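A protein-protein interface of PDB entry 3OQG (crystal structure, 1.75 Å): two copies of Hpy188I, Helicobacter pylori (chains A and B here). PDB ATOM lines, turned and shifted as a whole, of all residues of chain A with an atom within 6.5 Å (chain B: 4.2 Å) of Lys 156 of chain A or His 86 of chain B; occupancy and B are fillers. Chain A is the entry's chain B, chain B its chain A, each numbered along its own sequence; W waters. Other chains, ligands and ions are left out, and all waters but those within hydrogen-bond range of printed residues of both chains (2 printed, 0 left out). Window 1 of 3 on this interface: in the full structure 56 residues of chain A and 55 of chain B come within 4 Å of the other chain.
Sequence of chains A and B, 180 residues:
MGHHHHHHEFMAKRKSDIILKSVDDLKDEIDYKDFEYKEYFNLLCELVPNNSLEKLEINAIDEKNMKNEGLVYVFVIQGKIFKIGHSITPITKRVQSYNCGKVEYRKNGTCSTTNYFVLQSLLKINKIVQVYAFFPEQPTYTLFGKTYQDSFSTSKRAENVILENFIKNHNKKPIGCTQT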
ATOM      1  N   ILE A  88     -23.822 -25.831   9.337  1.00  0.00           N
ATOM      2  CA  ILE A  88     -22.657 -25.841  10.222  1.00  0.00           C
ATOM      3  C   ILE A  88     -22.889 -26.679  11.496  1.00  0.00           C
ATOM      4  O   ILE A  88     -21.962 -26.905  12.263  1.00  0.00           O
ATOM      5  CB  ILE A  88     -22.213 -24.407  10.610  1.00  0.00           C
ATOM      6  CG1 ILE A  88     -23.180 -23.778  11.629  1.00  0.00           C
ATOM      7  CG2 ILE A  88     -22.067 -23.544   9.342  1.00  0.00           C
ATOM      8  CD1 ILE A  88     -22.805 -22.344  12.041  1.00  0.00           C
ATOM      9  N   TYR A 141      -7.772 -22.160  11.713  1.00  0.00           N
ATOM     10  CA  TYR A 141      -7.673 -20.711  11.645  1.00  0.00           C
ATOM     11  C   TYR A 141      -7.377 -20.127  13.016  1.00  0.00           C
ATOM     12  O   TYR A 141      -7.579 -20.781  14.033  1.00  0.00           O
ATOM     13  CB  TYR A 141      -8.934 -20.101  11.025  1.00  0.00           C
ATOM     14  CG  TYR A 141     -10.243 -20.376  11.749  1.00  0.00           C
ATOM     15  CD1 TYR A 141     -10.787 -19.441  12.629  1.00  0.00           C
ATOM     16  CD2 TYR A 141     -10.954 -21.551  11.525  1.00  0.00           C
ATOM     17  CE1 TYR A 141     -12.004 -19.678  13.276  1.00  0.00           C
ATOM     18  CE2 TYR A 141     -12.170 -21.795  12.173  1.00  0.00           C
ATOM     19  CZ  TYR A 141     -12.688 -20.854  13.045  1.00  0.00           C
ATOM     20  OH  TYR A 141     -13.882 -21.102  13.680  1.00  0.00           O
ATOM     21  N   PHE A 152     -17.547 -23.369  11.586  1.00  0.00           N
ATOM     22  CA  PHE A 152     -18.019 -21.984  11.604  1.00  0.00           C
ATOM     23  C   PHE A 152     -17.260 -21.143  10.593  1.00  0.00           C
ATOM     24  O   PHE A 152     -16.065 -21.358  10.349  1.00  0.00           O
ATOM     25  CB  PHE A 152     -17.816 -21.360  12.998  1.00  0.00           C
ATOM     26  CG  PHE A 152     -18.881 -21.709  14.006  1.00  0.00           C
ATOM     27  CD1 PHE A 152     -19.468 -22.975  14.038  1.00  0.00           C
ATOM     28  CD2 PHE A 152     -19.247 -20.781  14.975  1.00  0.00           C
ATOM     29  CE1 PHE A 152     -20.447 -23.279  14.991  1.00  0.00           C
ATOM     30  CE2 PHE A 152     -20.209 -21.077  15.929  1.00  0.00           C
ATOM     31  CZ  PHE A 152     -20.808 -22.337  15.940  1.00  0.00           C
ATOM     32  N   SER A 153     -17.926 -20.144  10.044  1.00  0.00           N
ATOM     33  CA  SER A 153     -17.197 -19.064   9.361  1.00  0.00           C
ATOM     34  C   SER A 153     -16.335 -18.359  10.401  1.00  0.00           C
ATOM     35  O   SER A 153     -16.654 -18.376  11.588  1.00  0.00           O
ATOM     36  CB  SER A 153     -18.157 -18.079   8.716  1.00  0.00           C
ATOM     37  OG  SER A 153     -18.844 -17.317   9.700  1.00  0.00           O
ATOM     38  N   THR A 154     -15.235 -17.742   9.964  1.00  0.00           N
ATOM     39  CA  THR A 154     -14.354 -17.038  10.896  1.00  0.00           C
ATOM     40  C   THR A 154     -15.050 -15.864  11.589  1.00  0.00           C
ATOM     41  O   THR A 154     -14.818 -15.624  12.774  1.00  0.00           O
ATOM     42  CB  THR A 154     -13.044 -16.569  10.220  1.00  0.00           C
ATOM     43  OG1 THR A 154     -13.348 -15.767   9.068  1.00  0.00           O
ATOM     44  CG2 THR A 154     -12.191 -17.793   9.816  1.00  0.00           C
ATOM     45  N   SER A 155     -15.917 -15.152  10.869  1.00  0.00           N
ATOM     46  CA  SER A 155     -16.681 -14.049  11.473  1.00  0.00           C
ATOM     47  C   SER A 155     -17.677 -14.550  12.531  1.00  0.00           C
ATOM     48  O   SER A 155     -17.818 -13.922  13.594  1.00  0.00           O
ATOM     49  CB  SER A 155     -17.367 -13.175  10.408  1.00  0.00           C
ATOM     50  OG  SER A 155     -18.401 -13.839   9.709  1.00  0.00           O
ATOM     51  N   LYS A 156     -18.345 -15.678  12.263  1.00  0.00           N
ATOM     52  CA  LYS A 156     -19.271 -16.250  13.256  1.00  0.00           C
ATOM     53  C   LYS A 156     -18.513 -16.711  14.498  1.00  0.00           C
ATOM     54  O   LYS A 156     -18.946 -16.447  15.617  1.00  0.00           O
ATOM     55  CB  LYS A 156     -20.120 -17.386  12.693  1.00  0.00           C
ATOM     56  CG  LYS A 156     -21.090 -17.969  13.751  1.00  0.00           C
ATOM     57  CD  LYS A 156     -22.212 -18.802  13.138  1.00  0.00           C
ATOM     58  CE  LYS A 156     -22.997 -19.542  14.230  1.00  0.00           C
ATOM     59  NZ  LYS A 156     -23.722 -18.657  15.164  1.00  0.00           N
ATOM     60  N   ARG A 157     -17.386 -17.391  14.317  1.00  0.00           N
ATOM     61  CA  ARG A 157     -16.587 -17.830  15.457  1.00  0.00           C
ATOM     62  C   ARG A 157     -16.085 -16.611  16.230  1.00  0.00           C
ATOM     63  O   ARG A 157     -16.157 -16.590  17.459  1.00  0.00           O
ATOM     64  CB  ARG A 157     -15.418 -18.724  15.022  1.00  0.00           C
ATOM     65  CG  ARG A 157     -14.465 -19.126  16.152  1.00  0.00           C
ATOM     66  CD  ARG A 157     -15.196 -19.805  17.323  1.00  0.00           C
ATOM     67  NE  ARG A 157     -15.838 -21.061  16.918  1.00  0.00           N
ATOM     68  CZ  ARG A 157     -16.860 -21.640  17.548  1.00  0.00           C
ATOM     69  NH1 ARG A 157     -17.391 -21.091  18.637  1.00  0.00           N
ATOM     70  NH2 ARG A 157     -17.370 -22.774  17.075  1.00  0.00           N
ATOM     71  N   ALA A 158     -15.616 -15.598  15.501  1.00  0.00           N
ATOM     72  CA  ALA A 158     -15.130 -14.354  16.117  1.00  0.00           C
ATOM     73  C   ALA A 158     -16.230 -13.695  16.960  1.00  0.00           C
ATOM     74  O   ALA A 158     -15.979 -13.287  18.090  1.00  0.00           O
ATOM     75  CB  ALA A 158     -14.581 -13.386  15.041  1.00  0.00           C
ATOM     76  N   GLU A 159     -17.453 -13.635  16.429  1.00  0.00           N
ATOM     77  CA  GLU A 159     -18.587 -13.084  17.164  1.00  0.00           C
ATOM     78  C   GLU A 159     -18.859 -13.862  18.449  1.00  0.00           C
ATOM     79  O   GLU A 159     -19.064 -13.271  19.508  1.00  0.00           O
ATOM     80  CB  GLU A 159     -19.837 -13.122  16.297  1.00  0.00           C
ATOM     81  CG  GLU A 159     -21.113 -12.745  17.024  1.00  0.00           C
ATOM     82  CD  GLU A 159     -22.310 -13.284  16.307  1.00  0.00           C
ATOM     83  OE1 GLU A 159     -22.640 -14.462  16.543  1.00  0.00           O
ATOM     84  OE2 GLU A 159     -22.904 -12.553  15.478  1.00  0.00           O
ATOM     85  N   ASN A 160     -18.865 -15.180  18.338  1.00  0.00           N
ATOM     86  CA  ASN A 160     -19.152 -16.042  19.480  1.00  0.00           C
ATOM     87  C   ASN A 160     -18.123 -15.863  20.597  1.00  0.00           C
ATOM     88  O   ASN A 160     -18.488 -15.820  21.772  1.00  0.00           O
ATOM     89  CB  ASN A 160     -19.227 -17.501  19.016  1.00  0.00           C
ATOM     90  CG  ASN A 160     -19.430 -18.469  20.160  1.00  0.00           C
ATOM     91  OD1 ASN A 160     -18.481 -19.078  20.628  1.00  0.00           O
ATOM     92  ND2 ASN A 160     -20.663 -18.592  20.631  1.00  0.00           N
ATOM     93  N   VAL A 161     -16.846 -15.756  20.233  1.00  0.00           N
ATOM     94  CA  VAL A 161     -15.762 -15.571  21.194  1.00  0.00           C
ATOM     95  C   VAL A 161     -15.878 -14.220  21.892  1.00  0.00           C
ATOM     96  O   VAL A 161     -15.795 -14.126  23.116  1.00  0.00           O
ATOM     97  CB  VAL A 161     -14.392 -15.675  20.484  1.00  0.00           C
ATOM     98  CG1 VAL A 161     -13.256 -15.163  21.368  1.00  0.00           C
ATOM     99  CG2 VAL A 161     -14.147 -17.113  20.025  1.00  0.00           C
ATOM    100  N   THR A 180     -26.367 -16.480  21.284  1.00  0.00           N
ATOM    101  CA  THR A 180     -24.895 -16.402  21.367  1.00  0.00           C
ATOM    102  C   THR A 180     -24.292 -17.147  20.166  1.00  0.00           C
ATOM    103  O   THR A 180     -23.092 -17.037  19.889  1.00  0.00           O
ATOM    104  CB  THR A 180     -24.345 -17.029  22.666  1.00  0.00           C
ATOM    105  OG1 THR A 180     -24.681 -18.420  22.697  1.00  0.00           O
ATOM    106  CG2 THR A 180     -24.923 -16.330  23.906  1.00  0.00           C
ATOM    107  OXT THR A 180     -24.984 -17.878  19.440  1.00  0.00           O
ATOM    108  N   LEU B  71     -17.023  -9.935   8.626  1.00  0.00           N
ATOM    109  CA  LEU B  71     -16.723  -9.007   9.712  1.00  0.00           C
ATOM    110  C   LEU B  71     -17.558  -9.315  10.953  1.00  0.00           C
ATOM    111  O   LEU B  71     -18.646  -9.896  10.871  1.00  0.00           O
ATOM    112  CB  LEU B  71     -16.982  -7.552   9.293  1.00  0.00           C
ATOM    113  CG  LEU B  71     -18.426  -7.093   9.027  1.00  0.00           C
ATOM    114  CD1 LEU B  71     -18.558  -5.541   9.173  1.00  0.00           C
ATOM    115  CD2 LEU B  71     -18.846  -7.557   7.644  1.00  0.00           C
ATOM    116  N   TYR B  73     -19.283  -6.831  13.722  1.00  0.00           N
ATOM    117  CA  TYR B  73     -19.624  -5.421  13.902  1.00  0.00           C
ATOM    118  C   TYR B  73     -20.272  -5.137  15.242  1.00  0.00           C
ATOM    119  O   TYR B  73     -20.855  -6.034  15.881  1.00  0.00           O
ATOM    120  CB  TYR B  73     -20.515  -4.918  12.766  1.00  0.00           C
ATOM    121  CG  TYR B  73     -21.827  -5.644  12.640  1.00  0.00           C
ATOM    122  CD1 TYR B  73     -21.973  -6.694  11.759  1.00  0.00           C
ATOM    123  CD2 TYR B  73     -22.936  -5.255  13.397  1.00  0.00           C
ATOM    124  CE1 TYR B  73     -23.202  -7.374  11.634  1.00  0.00           C
ATOM    125  CE2 TYR B  73     -24.154  -5.878  13.267  1.00  0.00           C
ATOM    126  CZ  TYR B  73     -24.287  -6.942  12.405  1.00  0.00           C
ATOM    127  OH  TYR B  73     -25.484  -7.588  12.298  1.00  0.00           O
ATOM    128  N   GLY B  85     -22.821  -8.181  16.119  1.00  0.00           N
ATOM    129  CA  GLY B  85     -23.237  -9.149  15.108  1.00  0.00           C
ATOM    130  C   GLY B  85     -22.124  -9.518  14.159  1.00  0.00           C
ATOM    131  O   GLY B  85     -20.995  -9.068  14.306  1.00  0.00           O
ATOM    132  N   HIS B  86     -22.439 -10.343  13.169  1.00  0.00           N
ATOM    133  CA  HIS B  86     -21.464 -10.675  12.158  1.00  0.00           C
ATOM    134  C   HIS B  86     -22.141 -10.813  10.799  1.00  0.00           C
ATOM    135  O   HIS B  86     -23.376 -11.004  10.690  1.00  0.00           O
ATOM    136  CB  HIS B  86     -20.730 -11.976  12.515  1.00  0.00           C
ATOM    137  CG  HIS B  86     -21.492 -13.206  12.118  1.00  0.00           C
ATOM    138  ND1 HIS B  86     -22.515 -13.728  12.881  1.00  0.00           N
ATOM    139  CD2 HIS B  86     -21.444 -13.956  10.993  1.00  0.00           C
ATOM    140  CE1 HIS B  86     -23.019 -14.784  12.272  1.00  0.00           C
ATOM    141  NE2 HIS B  86     -22.407 -14.929  11.112  1.00  0.00           N
ATOM    142  N   SER B  87     -21.311 -10.773   9.769  1.00  0.00           N
ATOM    143  CA  SER B  87     -21.747 -11.014   8.412  1.00  0.00           C
ATOM    144  C   SER B  87     -20.626 -11.597   7.565  1.00  0.00           C
ATOM    145  O   SER B  87     -19.477 -11.139   7.653  1.00  0.00           O
ATOM    146  CB  SER B  87     -22.221  -9.738   7.749  1.00  0.00           C
ATOM    147  OG  SER B  87     -22.722 -10.010   6.443  1.00  0.00           O
HETATM  148  O   HOH W   1     -21.599 -17.244   9.147  1.00  0.00           O
HETATM  149  O   HOH W   2     -24.993 -15.017  14.770  1.00  0.00           O
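Of the 5 printed residues of chain B, 4 touch a printed residue of chain A. Hydrophobic or aromatic side chains of chain B that line the printed part of chain A: His 86. Among the printed residues, 6 pairs touch across the chains.
Among the printed residues, merely in contact across the chains: Ser 155 of chain A with His 86 of chain B, Glu 159 of chain A with Gly 85 of chain B, Ser 155 of chain A with Leu 71 of chain B, Ser 155 of chain A with Ser 87 of chain B and Lys 156 of chain A with His 86 of chain B.
Thr 154 of chain A touches none of the printed residues of chain B. Printed residues of chain B within 4 Å of Ser 155 of chain A: Leu 71 (3.5 Å), His 86 (3.3 Å) and Ser 87 (3.6 Å). Lys 156 of chain A touches one residue of chain B. Printed residues of chain A within 4 Å of Gly 85 of chain B: Glu 159 (3.4 Å). Of chain A, only Ser 155 (3.3 Å), Lys 156 (3.7 Å) and Glu 159 (2.9 Å) come within 4 Å of His 86 of chain B. Of the printed residues of chain A, Ser 87 of chain B touches Ser 155. The nearest residue of chain A that does not touch His 86 of chain B is Ser 153 of chain A (4.4 Å). The nearest printed residue of chain B that does not touch Glu 159 of chain A is Ser 87 of chain B (6.2 Å).
No position is printed for both chains. Of the 6 pairs that touch across the chains among the printed residues, none has its exchanged pair printed and touching as well.
ND1 of His 86 of chain B sits at hydrogen-bond distance from OE2 of Glu 159 of chain A, 2.9 Å away.
The backbone NH of Leu 71 of chain B lies within hydrogen-bond range of the backbone carbonyl oxygen of Ser 87 of chain B, 2.9 Å away. O of Gly 85 of chain B is in hydrogen-bond range of N of Tyr 73 of chain B (2.9 Å). OG of Ser 153 of chain A sits at hydrogen-bond distance from N of Lys 156 of chain A, at 3.1 Å.
Water W1 bridges the side-chain hydroxyl of Ser 153 of chain A and a ring nitrogen (NE2) of His 86 of chain B. Water W2 bridges the side-chain carboxylate (OE1) of Glu 159 of chain A (3.0 Å) and a ring nitrogen (ND1) of His 86 of chain B (3.4 Å).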
